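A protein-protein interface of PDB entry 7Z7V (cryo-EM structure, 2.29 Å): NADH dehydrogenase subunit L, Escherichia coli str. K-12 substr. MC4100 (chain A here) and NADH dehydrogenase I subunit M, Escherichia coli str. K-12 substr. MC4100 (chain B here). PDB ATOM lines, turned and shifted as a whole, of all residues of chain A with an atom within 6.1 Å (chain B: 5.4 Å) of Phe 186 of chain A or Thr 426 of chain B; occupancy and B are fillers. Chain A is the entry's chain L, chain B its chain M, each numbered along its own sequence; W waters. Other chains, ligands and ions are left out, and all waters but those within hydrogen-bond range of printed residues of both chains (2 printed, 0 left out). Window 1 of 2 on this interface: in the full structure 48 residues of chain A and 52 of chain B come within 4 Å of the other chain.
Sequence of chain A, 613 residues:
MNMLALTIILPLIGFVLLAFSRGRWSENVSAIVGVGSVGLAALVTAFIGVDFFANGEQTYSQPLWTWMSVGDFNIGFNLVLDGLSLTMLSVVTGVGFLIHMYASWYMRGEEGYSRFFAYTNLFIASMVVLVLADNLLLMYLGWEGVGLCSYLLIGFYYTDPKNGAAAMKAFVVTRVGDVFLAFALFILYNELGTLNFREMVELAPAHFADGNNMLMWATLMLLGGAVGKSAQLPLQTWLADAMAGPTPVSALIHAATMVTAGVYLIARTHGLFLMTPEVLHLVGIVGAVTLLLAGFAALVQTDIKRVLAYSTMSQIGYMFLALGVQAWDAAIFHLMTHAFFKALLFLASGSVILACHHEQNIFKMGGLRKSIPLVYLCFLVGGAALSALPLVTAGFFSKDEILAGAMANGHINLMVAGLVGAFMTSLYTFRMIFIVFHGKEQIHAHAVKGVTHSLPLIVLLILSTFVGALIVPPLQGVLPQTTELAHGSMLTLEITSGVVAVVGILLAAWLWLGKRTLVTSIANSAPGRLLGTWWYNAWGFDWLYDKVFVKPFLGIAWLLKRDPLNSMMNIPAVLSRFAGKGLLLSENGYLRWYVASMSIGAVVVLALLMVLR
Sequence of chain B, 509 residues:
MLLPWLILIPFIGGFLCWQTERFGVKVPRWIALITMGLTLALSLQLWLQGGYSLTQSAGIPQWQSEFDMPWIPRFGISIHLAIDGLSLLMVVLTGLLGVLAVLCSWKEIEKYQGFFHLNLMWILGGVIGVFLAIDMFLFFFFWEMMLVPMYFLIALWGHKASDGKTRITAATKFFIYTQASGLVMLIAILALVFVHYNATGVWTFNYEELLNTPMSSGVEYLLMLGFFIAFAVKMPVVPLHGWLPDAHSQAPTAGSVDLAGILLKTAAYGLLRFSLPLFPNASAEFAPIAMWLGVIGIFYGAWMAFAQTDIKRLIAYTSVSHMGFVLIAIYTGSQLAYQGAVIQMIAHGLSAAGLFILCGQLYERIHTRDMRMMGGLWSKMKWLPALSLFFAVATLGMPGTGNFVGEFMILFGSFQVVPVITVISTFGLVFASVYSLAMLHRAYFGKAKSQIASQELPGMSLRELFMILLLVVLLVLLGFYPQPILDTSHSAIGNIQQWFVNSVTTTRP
Phe 186 of chain A touches four residues of chain B.
Printed residues of chain B within 4 Å of Tyr 189 of chain A: Phe 412.
Phe 325 of chain B touches none of the printed residues of chain A.
Of the printed residues of chain A, Phe 408 of chain B touches Tyr 140 and Ala 182.
Ser 425 of chain B touches none of the printed residues of chain A.
Thr 426 of chain B touches just these residues of chain A: Val 179, Phe 183 and Phe 186.
Of the 15 printed residues of chain A, 9 touch a printed residue of chain B.
Of the 15 printed residues of chain B, 8 touch a printed residue of chain A.
Printed residues of chain B that touch a printed residue of chain A: Phe 408, Leu 411, Phe 412, Phe 415, Val 423, Thr 426, Phe 427 and Val 430.
Hydrophobic or aromatic side chains of chain B that line the printed part of chain A: Phe 408, Leu 411, Phe 412, Phe 415, Val 423, Phe 427 and Val 430.
Along chain B the printed residues that touch a printed residue of chain A span positions 408 to 430.
Among the printed residues, no Asp or Glu carboxylate lies within 4 Å of a Lys or Arg side-chain nitrogen of the other chain.
Val 179 of chain A touches Thr 426 of chain B (CG2 to O, 3.3 Å).
CE1 of Phe 427 of chain B touches CG1 of Val 179 of chain A, 3.6 Å away.
CB of Ala 182 of chain A touches CZ of Phe 408 of chain B, 3.6 Å away.
Thr 426 of chain B touches Phe 183 of chain A (OG1 to CE1, 3.4 Å).
CZ of Phe 183 of chain A touches CE2 of Phe 427 of chain B, 3.8 Å away.
Leu 185 of chain A touches Phe 412 of chain B.
Phe 186 of chain A touches Phe 412 of chain B (CD1 to CE1, 3.5 Å).
Phe 186 of chain A touches Phe 415 of chain B (CB to CG, 3.7 Å).
OG1 of Thr 426 of chain B touches CE2 of Phe 186 of chain A, at 3.9 Å.
Leu 195 of chain A touches Phe 412 of chain B (CD1 to CZ, 3.7 Å).
Water W1 lies within hydrogen-bond range of the backbone carbonyl oxygen (O) of Phe 415 of chain B (2.9 Å) and the side-chain amide nitrogen (ND2) of Asn 190 of chain A (3.4 Å).
Water W2 lies within hydrogen-bond range of O of Phe 186 of chain A (3.0 Å) and O of Phe 412 of chain B (3.0 Å).
The backbone NH of Phe 415 of chain B sits at hydrogen-bond distance from the side-chain hydroxyl of Thr 422 of chain B (3.1 Å).
OG1 of Thr 426 of chain B sits at hydrogen-bond distance from O of Thr 422 of chain B (2.6 Å).
The backbone carbonyl oxygen (O) of Asp 178 of chain A is in hydrogen-bond range of the side-chain hydroxyl (OH) of Tyr 140 of chain A (2.8 Å).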
ATOM      1  N   TYR A 140      -3.732 -21.622  28.503  1.00  0.00           N
ATOM      2  CA  TYR A 140      -5.012 -21.008  28.170  1.00  0.00           C
ATOM      3  C   TYR A 140      -6.178 -21.830  28.707  1.00  0.00           C
ATOM      4  O   TYR A 140      -7.197 -21.267  29.119  1.00  0.00           O
ATOM      5  CB  TYR A 140      -5.124 -20.836  26.656  1.00  0.00           C
ATOM      6  CG  TYR A 140      -6.151 -19.824  26.219  1.00  0.00           C
ATOM      7  CD1 TYR A 140      -5.809 -18.492  26.046  1.00  0.00           C
ATOM      8  CD2 TYR A 140      -7.461 -20.203  25.970  1.00  0.00           C
ATOM      9  CE1 TYR A 140      -6.745 -17.565  25.643  1.00  0.00           C
ATOM     10  CE2 TYR A 140      -8.400 -19.285  25.566  1.00  0.00           C
ATOM     11  CZ  TYR A 140      -8.039 -17.968  25.406  1.00  0.00           C
ATOM     12  OH  TYR A 140      -8.979 -17.054  25.003  1.00  0.00           O
ATOM     13  N   ASP A 178      -9.008 -12.559  27.799  1.00  0.00           N
ATOM     14  CA  ASP A 178      -8.686 -13.843  27.179  1.00  0.00           C
ATOM     15  C   ASP A 178      -8.645 -13.743  25.663  1.00  0.00           C
ATOM     16  O   ASP A 178      -7.894 -14.475  25.018  1.00  0.00           O
ATOM     17  CB  ASP A 178      -9.698 -14.906  27.598  1.00  0.00           C
ATOM     18  CG  ASP A 178      -9.846 -15.007  29.094  1.00  0.00           C
ATOM     19  OD1 ASP A 178      -8.953 -14.518  29.812  1.00  0.00           O
ATOM     20  OD2 ASP A 178     -10.871 -15.538  29.565  1.00  0.00           O
ATOM     21  N   VAL A 179      -9.449 -12.857  25.083  1.00  0.00           N
ATOM     22  CA  VAL A 179      -9.400 -12.633  23.643  1.00  0.00           C
ATOM     23  C   VAL A 179      -8.081 -11.976  23.249  1.00  0.00           C
ATOM     24  O   VAL A 179      -7.467 -12.336  22.234  1.00  0.00           O
ATOM     25  CB  VAL A 179     -10.629 -11.812  23.214  1.00  0.00           C
ATOM     26  CG1 VAL A 179     -10.360 -10.984  21.981  1.00  0.00           C
ATOM     27  CG2 VAL A 179     -11.785 -12.742  22.980  1.00  0.00           C
ATOM     28  N   LEU A 181      -5.308 -12.414  24.952  1.00  0.00           N
ATOM     29  CA  LEU A 181      -4.362 -13.517  25.111  1.00  0.00           C
ATOM     30  C   LEU A 181      -4.404 -14.467  23.915  1.00  0.00           C
ATOM     31  O   LEU A 181      -3.365 -14.976  23.476  1.00  0.00           O
ATOM     32  CB  LEU A 181      -4.662 -14.267  26.405  1.00  0.00           C
ATOM     33  CG  LEU A 181      -3.769 -15.444  26.778  1.00  0.00           C
ATOM     34  CD1 LEU A 181      -2.309 -15.036  26.779  1.00  0.00           C
ATOM     35  CD2 LEU A 181      -4.180 -15.974  28.129  1.00  0.00           C
ATOM     36  N   ALA A 182      -5.598 -14.707  23.374  1.00  0.00           N
ATOM     37  CA  ALA A 182      -5.736 -15.533  22.182  1.00  0.00           C
ATOM     38  C   ALA A 182      -5.056 -14.889  20.984  1.00  0.00           C
ATOM     39  O   ALA A 182      -4.468 -15.586  20.154  1.00  0.00           O
ATOM     40  CB  ALA A 182      -7.212 -15.785  21.885  1.00  0.00           C
ATOM     41  N   PHE A 183      -5.131 -13.559  20.880  1.00  0.00           N
ATOM     42  CA  PHE A 183      -4.399 -12.853  19.827  1.00  0.00           C
ATOM     43  C   PHE A 183      -2.902 -13.079  19.955  1.00  0.00           C
ATOM     44  O   PHE A 183      -2.211 -13.307  18.951  1.00  0.00           O
ATOM     45  CB  PHE A 183      -4.686 -11.355  19.879  1.00  0.00           C
ATOM     46  CG  PHE A 183      -6.091 -10.990  19.550  1.00  0.00           C
ATOM     47  CD1 PHE A 183      -6.909 -11.864  18.862  1.00  0.00           C
ATOM     48  CD2 PHE A 183      -6.600  -9.763  19.938  1.00  0.00           C
ATOM     49  CE1 PHE A 183      -8.194 -11.527  18.572  1.00  0.00           C
ATOM     50  CE2 PHE A 183      -7.896  -9.420  19.642  1.00  0.00           C
ATOM     51  CZ  PHE A 183      -8.693 -10.303  18.956  1.00  0.00           C
ATOM     52  N   ALA A 184      -2.389 -13.011  21.186  1.00  0.00           N
ATOM     53  CA  ALA A 184      -0.973 -13.292  21.421  1.00  0.00           C
ATOM     54  C   ALA A 184      -0.612 -14.708  20.990  1.00  0.00           C
ATOM     55  O   ALA A 184       0.427 -14.927  20.356  1.00  0.00           O
ATOM     56  CB  ALA A 184      -0.629 -13.089  22.894  1.00  0.00           C
ATOM     57  N   LEU A 185      -1.474 -15.675  21.314  1.00  0.00           N
ATOM     58  CA  LEU A 185      -1.235 -17.064  20.929  1.00  0.00           C
ATOM     59  C   LEU A 185      -1.234 -17.238  19.412  1.00  0.00           C
ATOM     60  O   LEU A 185      -0.393 -17.966  18.868  1.00  0.00           O
ATOM     61  CB  LEU A 185      -2.289 -17.967  21.570  1.00  0.00           C
ATOM     62  CG  LEU A 185      -1.888 -18.723  22.836  1.00  0.00           C
ATOM     63  CD1 LEU A 185      -1.791 -17.782  24.014  1.00  0.00           C
ATOM     64  CD2 LEU A 185      -2.882 -19.822  23.130  1.00  0.00           C
ATOM     65  N   PHE A 186      -2.165 -16.574  18.716  1.00  0.00           N
ATOM     66  CA  PHE A 186      -2.233 -16.681  17.258  1.00  0.00           C
ATOM     67  C   PHE A 186      -0.990 -16.093  16.607  1.00  0.00           C
ATOM     68  O   PHE A 186      -0.416 -16.703  15.696  1.00  0.00           O
ATOM     69  CB  PHE A 186      -3.475 -15.975  16.702  1.00  0.00           C
ATOM     70  CG  PHE A 186      -4.779 -16.458  17.269  1.00  0.00           C
ATOM     71  CD1 PHE A 186      -4.924 -17.748  17.750  1.00  0.00           C
ATOM     72  CD2 PHE A 186      -5.869 -15.607  17.316  1.00  0.00           C
ATOM     73  CE1 PHE A 186      -6.120 -18.172  18.277  1.00  0.00           C
ATOM     74  CE2 PHE A 186      -7.068 -16.027  17.837  1.00  0.00           C
ATOM     75  CZ  PHE A 186      -7.191 -17.310  18.324  1.00  0.00           C
ATOM     76  N   ILE A 187      -0.556 -14.916  17.073  1.00  0.00           N
ATOM     77  CA  ILE A 187       0.644 -14.284  16.529  1.00  0.00           C
ATOM     78  C   ILE A 187       1.869 -15.152  16.781  1.00  0.00           C
ATOM     79  O   ILE A 187       2.701 -15.351  15.887  1.00  0.00           O
ATOM     80  CB  ILE A 187       0.825 -12.873  17.121  1.00  0.00           C
ATOM     81  CG1 ILE A 187      -0.310 -11.952  16.689  1.00  0.00           C
ATOM     82  CG2 ILE A 187       2.152 -12.273  16.698  1.00  0.00           C
ATOM     83  CD1 ILE A 187      -0.411 -10.696  17.510  1.00  0.00           C
ATOM     84  N   LEU A 188       1.987 -15.699  17.993  1.00  0.00           N
ATOM     85  CA  LEU A 188       3.178 -16.466  18.338  1.00  0.00           C
ATOM     86  C   LEU A 188       3.241 -17.782  17.575  1.00  0.00           C
ATOM     87  O   LEU A 188       4.328 -18.212  17.171  1.00  0.00           O
ATOM     88  CB  LEU A 188       3.224 -16.702  19.845  1.00  0.00           C
ATOM     89  CG  LEU A 188       3.731 -15.482  20.614  1.00  0.00           C
ATOM     90  CD1 LEU A 188       3.522 -15.647  22.103  1.00  0.00           C
ATOM     91  CD2 LEU A 188       5.190 -15.221  20.297  1.00  0.00           C
ATOM     92  N   TYR A 189       2.096 -18.434  17.349  1.00  0.00           N
ATOM     93  CA  TYR A 189       2.123 -19.642  16.532  1.00  0.00           C
ATOM     94  C   TYR A 189       2.401 -19.316  15.070  1.00  0.00           C
ATOM     95  O   TYR A 189       3.124 -20.058  14.396  1.00  0.00           O
ATOM     96  CB  TYR A 189       0.820 -20.426  16.647  1.00  0.00           C
ATOM     97  CG  TYR A 189       0.771 -21.554  15.644  1.00  0.00           C
ATOM     98  CD1 TYR A 189       1.635 -22.636  15.754  1.00  0.00           C
ATOM     99  CD2 TYR A 189      -0.095 -21.514  14.560  1.00  0.00           C
ATOM    100  CE1 TYR A 189       1.617 -23.658  14.833  1.00  0.00           C
ATOM    101  CE2 TYR A 189      -0.116 -22.531  13.631  1.00  0.00           C
ATOM    102  CZ  TYR A 189       0.742 -23.600  13.773  1.00  0.00           C
ATOM    103  OH  TYR A 189       0.720 -24.618  12.853  1.00  0.00           O
ATOM    104  N   ASN A 190       1.830 -18.222  14.557  1.00  0.00           N
ATOM    105  CA  ASN A 190       2.057 -17.861  13.162  1.00  0.00           C
ATOM    106  C   ASN A 190       3.508 -17.480  12.903  1.00  0.00           C
ATOM    107  O   ASN A 190       4.023 -17.726  11.808  1.00  0.00           O
ATOM    108  CB  ASN A 190       1.133 -16.714  12.759  1.00  0.00           C
ATOM    109  CG  ASN A 190       1.191 -16.415  11.279  1.00  0.00           C
ATOM    110  OD1 ASN A 190       1.123 -17.317  10.450  1.00  0.00           O
ATOM    111  ND2 ASN A 190       1.326 -15.142  10.939  1.00  0.00           N
ATOM    112  N   GLU A 191       4.182 -16.896  13.890  1.00  0.00           N
ATOM    113  CA  GLU A 191       5.576 -16.505  13.707  1.00  0.00           C
ATOM    114  C   GLU A 191       6.535 -17.655  14.003  1.00  0.00           C
ATOM    115  O   GLU A 191       7.312 -18.062  13.135  1.00  0.00           O
ATOM    116  CB  GLU A 191       5.905 -15.297  14.590  1.00  0.00           C
ATOM    117  CG  GLU A 191       5.162 -14.026  14.219  1.00  0.00           C
ATOM    118  CD  GLU A 191       5.388 -13.605  12.787  1.00  0.00           C
ATOM    119  OE1 GLU A 191       6.545 -13.656  12.325  1.00  0.00           O
ATOM    120  OE2 GLU A 191       4.407 -13.218  12.121  1.00  0.00           O
ATOM    121  N   LEU A 195       4.097 -23.013  20.577  1.00  0.00           N
ATOM    122  CA  LEU A 195       3.592 -22.303  21.739  1.00  0.00           C
ATOM    123  C   LEU A 195       4.288 -22.721  23.023  1.00  0.00           C
ATOM    124  O   LEU A 195       3.954 -22.196  24.090  1.00  0.00           O
ATOM    125  CB  LEU A 195       2.079 -22.506  21.875  1.00  0.00           C
ATOM    126  CG  LEU A 195       1.222 -21.813  20.816  1.00  0.00           C
ATOM    127  CD1 LEU A 195      -0.254 -22.063  21.068  1.00  0.00           C
ATOM    128  CD2 LEU A 195       1.518 -20.325  20.768  1.00  0.00           C
ATOM    129  N   PHE B 325     -18.693 -19.122  12.271  1.00  0.00           N
ATOM    130  CA  PHE B 325     -17.295 -19.524  12.475  1.00  0.00           C
ATOM    131  C   PHE B 325     -16.862 -20.598  11.476  1.00  0.00           C
ATOM    132  O   PHE B 325     -15.770 -20.524  10.892  1.00  0.00           O
ATOM    133  CB  PHE B 325     -17.086 -20.036  13.897  1.00  0.00           C
ATOM    134  CG  PHE B 325     -16.834 -18.959  14.890  1.00  0.00           C
ATOM    135  CD1 PHE B 325     -15.596 -18.351  14.969  1.00  0.00           C
ATOM    136  CD2 PHE B 325     -17.841 -18.547  15.743  1.00  0.00           C
ATOM    137  CE1 PHE B 325     -15.369 -17.357  15.882  1.00  0.00           C
ATOM    138  CE2 PHE B 325     -17.617 -17.552  16.656  1.00  0.00           C
ATOM    139  CZ  PHE B 325     -16.382 -16.954  16.722  1.00  0.00           C
ATOM    140  N   PHE B 408     -10.986 -22.701  18.179  1.00  0.00           N
ATOM    141  CA  PHE B 408      -9.642 -22.170  18.334  1.00  0.00           C
ATOM    142  C   PHE B 408      -8.694 -22.670  17.254  1.00  0.00           C
ATOM    143  O   PHE B 408      -7.835 -21.905  16.809  1.00  0.00           O
ATOM    144  CB  PHE B 408      -9.104 -22.480  19.725  1.00  0.00           C
ATOM    145  CG  PHE B 408      -8.996 -21.267  20.590  1.00  0.00           C
ATOM    146  CD1 PHE B 408     -10.139 -20.628  21.042  1.00  0.00           C
ATOM    147  CD2 PHE B 408      -7.762 -20.743  20.927  1.00  0.00           C
ATOM    148  CE1 PHE B 408     -10.052 -19.501  21.829  1.00  0.00           C
ATOM    149  CE2 PHE B 408      -7.669 -19.616  21.714  1.00  0.00           C
ATOM    150  CZ  PHE B 408      -8.816 -18.994  22.162  1.00  0.00           C
ATOM    151  N   LEU B 411      -9.564 -20.459  14.397  1.00  0.00           N
ATOM    152  CA  LEU B 411      -8.985 -19.126  14.498  1.00  0.00           C
ATOM    153  C   LEU B 411      -7.476 -19.140  14.288  1.00  0.00           C
ATOM    154  O   LEU B 411      -6.934 -18.185  13.729  1.00  0.00           O
ATOM    155  CB  LEU B 411      -9.341 -18.507  15.847  1.00  0.00           C
ATOM    156  CG  LEU B 411     -10.806 -18.130  16.079  1.00  0.00           C
ATOM    157  CD1 LEU B 411     -11.013 -17.651  17.499  1.00  0.00           C
ATOM    158  CD2 LEU B 411     -11.285 -17.091  15.083  1.00  0.00           C
ATOM    159  N   PHE B 412      -6.788 -20.211  14.697  1.00  0.00           N
ATOM    160  CA  PHE B 412      -5.356 -20.330  14.424  1.00  0.00           C
ATOM    161  C   PHE B 412      -5.081 -20.373  12.922  1.00  0.00           C
ATOM    162  O   PHE B 412      -4.267 -19.593  12.400  1.00  0.00           O
ATOM    163  CB  PHE B 412      -4.799 -21.582  15.106  1.00  0.00           C
ATOM    164  CG  PHE B 412      -4.220 -21.336  16.473  1.00  0.00           C
ATOM    165  CD1 PHE B 412      -3.080 -20.571  16.633  1.00  0.00           C
ATOM    166  CD2 PHE B 412      -4.809 -21.889  17.597  1.00  0.00           C
ATOM    167  CE1 PHE B 412      -2.549 -20.353  17.888  1.00  0.00           C
ATOM    168  CE2 PHE B 412      -4.284 -21.671  18.855  1.00  0.00           C
ATOM    169  CZ  PHE B 412      -3.152 -20.904  19.001  1.00  0.00           C
ATOM    170  N   PHE B 415      -6.093 -16.967  11.266  1.00  0.00           N
ATOM    171  CA  PHE B 415      -5.078 -15.943  11.479  1.00  0.00           C
ATOM    172  C   PHE B 415      -3.856 -16.190  10.616  1.00  0.00           C
ATOM    173  O   PHE B 415      -3.210 -15.235  10.173  1.00  0.00           O
ATOM    174  CB  PHE B 415      -4.663 -15.876  12.946  1.00  0.00           C
ATOM    175  CG  PHE B 415      -3.863 -14.654  13.278  1.00  0.00           C
ATOM    176  CD1 PHE B 415      -4.495 -13.463  13.578  1.00  0.00           C
ATOM    177  CD2 PHE B 415      -2.477 -14.689  13.264  1.00  0.00           C
ATOM    178  CE1 PHE B 415      -3.763 -12.336  13.871  1.00  0.00           C
ATOM    179  CE2 PHE B 415      -1.744 -13.565  13.552  1.00  0.00           C
ATOM    180  CZ  PHE B 415      -2.387 -12.388  13.854  1.00  0.00           C
ATOM    181  N   ILE B 421     -10.248 -10.641   9.959  1.00  0.00           N
ATOM    182  CA  ILE B 421     -11.450 -11.446  10.147  1.00  0.00           C
ATOM    183  C   ILE B 421     -11.324 -12.297  11.405  1.00  0.00           C
ATOM    184  O   ILE B 421     -12.283 -12.448  12.173  1.00  0.00           O
ATOM    185  CB  ILE B 421     -11.702 -12.293   8.884  1.00  0.00           C
ATOM    186  CG1 ILE B 421     -12.193 -11.399   7.744  1.00  0.00           C
ATOM    187  CG2 ILE B 421     -12.689 -13.419   9.138  1.00  0.00           C
ATOM    188  CD1 ILE B 421     -11.623 -11.754   6.399  1.00  0.00           C
ATOM    189  N   THR B 422     -10.116 -12.805  11.667  1.00  0.00           N
ATOM    190  CA  THR B 422      -9.871 -13.620  12.853  1.00  0.00           C
ATOM    191  C   THR B 422     -10.052 -12.827  14.144  1.00  0.00           C
ATOM    192  O   THR B 422     -10.671 -13.321  15.099  1.00  0.00           O
ATOM    193  CB  THR B 422      -8.464 -14.207  12.785  1.00  0.00           C
ATOM    194  OG1 THR B 422      -8.289 -14.864  11.528  1.00  0.00           O
ATOM    195  CG2 THR B 422      -8.246 -15.199  13.902  1.00  0.00           C
ATOM    196  N   VAL B 423      -9.516 -11.603  14.203  1.00  0.00           N
ATOM    197  CA  VAL B 423      -9.617 -10.848  15.450  1.00  0.00           C
ATOM    198  C   VAL B 423     -11.065 -10.427  15.707  1.00  0.00           C
ATOM    199  O   VAL B 423     -11.556 -10.487  16.853  1.00  0.00           O
ATOM    200  CB  VAL B 423      -8.623  -9.661  15.475  1.00  0.00           C
ATOM    201  CG1 VAL B 423      -7.202 -10.154  15.255  1.00  0.00           C
ATOM    202  CG2 VAL B 423      -8.956  -8.562  14.493  1.00  0.00           C
ATOM    203  N   ILE B 424     -11.797 -10.086  14.639  1.00  0.00           N
ATOM    204  CA  ILE B 424     -13.211  -9.760  14.802  1.00  0.00           C
ATOM    205  C   ILE B 424     -13.994 -10.990  15.268  1.00  0.00           C
ATOM    206  O   ILE B 424     -14.851 -10.900  16.159  1.00  0.00           O
ATOM    207  CB  ILE B 424     -13.759  -9.157  13.494  1.00  0.00           C
ATOM    208  CG1 ILE B 424     -12.974  -7.894  13.146  1.00  0.00           C
ATOM    209  CG2 ILE B 424     -15.193  -8.760  13.641  1.00  0.00           C
ATOM    210  CD1 ILE B 424     -13.116  -7.453  11.712  1.00  0.00           C
ATOM    211  N   SER B 425     -13.651 -12.172  14.750  1.00  0.00           N
ATOM    212  CA  SER B 425     -14.334 -13.393  15.183  1.00  0.00           C
ATOM    213  C   SER B 425     -14.046 -13.745  16.646  1.00  0.00           C
ATOM    214  O   SER B 425     -14.925 -14.269  17.347  1.00  0.00           O
ATOM    215  CB  SER B 425     -13.940 -14.541  14.260  1.00  0.00           C
ATOM    216  OG  SER B 425     -13.868 -14.096  12.921  1.00  0.00           O
ATOM    217  N   THR B 426     -12.838 -13.464  17.132  1.00  0.00           N
ATOM    218  CA  THR B 426     -12.557 -13.717  18.547  1.00  0.00           C
ATOM    219  C   THR B 426     -13.381 -12.792  19.449  1.00  0.00           C
ATOM    220  O   THR B 426     -13.871 -13.203  20.522  1.00  0.00           O
ATOM    221  CB  THR B 426     -11.062 -13.564  18.807  1.00  0.00           C
ATOM    222  OG1 THR B 426     -10.342 -13.947  17.632  1.00  0.00           O
ATOM    223  CG2 THR B 426     -10.625 -14.462  19.942  1.00  0.00           C
ATOM    224  N   PHE B 427     -13.590 -11.549  19.016  1.00  0.00           N
ATOM    225  CA  PHE B 427     -14.567 -10.730  19.737  1.00  0.00           C
ATOM    226  C   PHE B 427     -15.976 -11.325  19.640  1.00  0.00           C
ATOM    227  O   PHE B 427     -16.800 -11.158  20.556  1.00  0.00           O
ATOM    228  CB  PHE B 427     -14.505  -9.296  19.230  1.00  0.00           C
ATOM    229  CG  PHE B 427     -13.274  -8.572  19.679  1.00  0.00           C
ATOM    230  CD1 PHE B 427     -13.028  -8.383  21.030  1.00  0.00           C
ATOM    231  CD2 PHE B 427     -12.340  -8.124  18.767  1.00  0.00           C
ATOM    232  CE1 PHE B 427     -11.891  -7.734  21.456  1.00  0.00           C
ATOM    233  CE2 PHE B 427     -11.198  -7.475  19.188  1.00  0.00           C
ATOM    234  CZ  PHE B 427     -10.975  -7.280  20.537  1.00  0.00           C
ATOM    235  N   GLY B 428     -16.244 -12.068  18.567  1.00  0.00           N
ATOM    236  CA  GLY B 428     -17.454 -12.880  18.526  1.00  0.00           C
ATOM    237  C   GLY B 428     -17.517 -13.924  19.632  1.00  0.00           C
ATOM    238  O   GLY B 428     -18.596 -14.236  20.142  1.00  0.00           O
ATOM    239  N   LEU B 429     -16.365 -14.495  19.997  1.00  0.00           N
ATOM    240  CA  LEU B 429     -16.330 -15.409  21.152  1.00  0.00           C
ATOM    241  C   LEU B 429     -16.731 -14.700  22.446  1.00  0.00           C
ATOM    242  O   LEU B 429     -17.411 -15.287  23.308  1.00  0.00           O
ATOM    243  CB  LEU B 429     -14.946 -16.039  21.328  1.00  0.00           C
ATOM    244  CG  LEU B 429     -14.264 -16.843  20.232  1.00  0.00           C
ATOM    245  CD1 LEU B 429     -12.976 -17.411  20.773  1.00  0.00           C
ATOM    246  CD2 LEU B 429     -15.176 -17.978  19.849  1.00  0.00           C
ATOM    247  N   VAL B 430     -16.292 -13.448  22.610  1.00  0.00           N
ATOM    248  CA  VAL B 430     -16.773 -12.645  23.748  1.00  0.00           C
ATOM    249  C   VAL B 430     -18.302 -12.522  23.726  1.00  0.00           C
ATOM    250  O   VAL B 430     -18.980 -12.694  24.757  1.00  0.00           O
ATOM    251  CB  VAL B 430     -16.095 -11.261  23.773  1.00  0.00           C
ATOM    252  CG1 VAL B 430     -16.933 -10.251  24.537  1.00  0.00           C
ATOM    253  CG2 VAL B 430     -14.758 -11.354  24.442  1.00  0.00           C
HETATM  254  O   HOH W   1      -1.016 -13.688   8.971  1.00  0.00           O
HETATM  255  O   HOH W   2      -1.802 -18.428  13.674  1.00  0.00           O
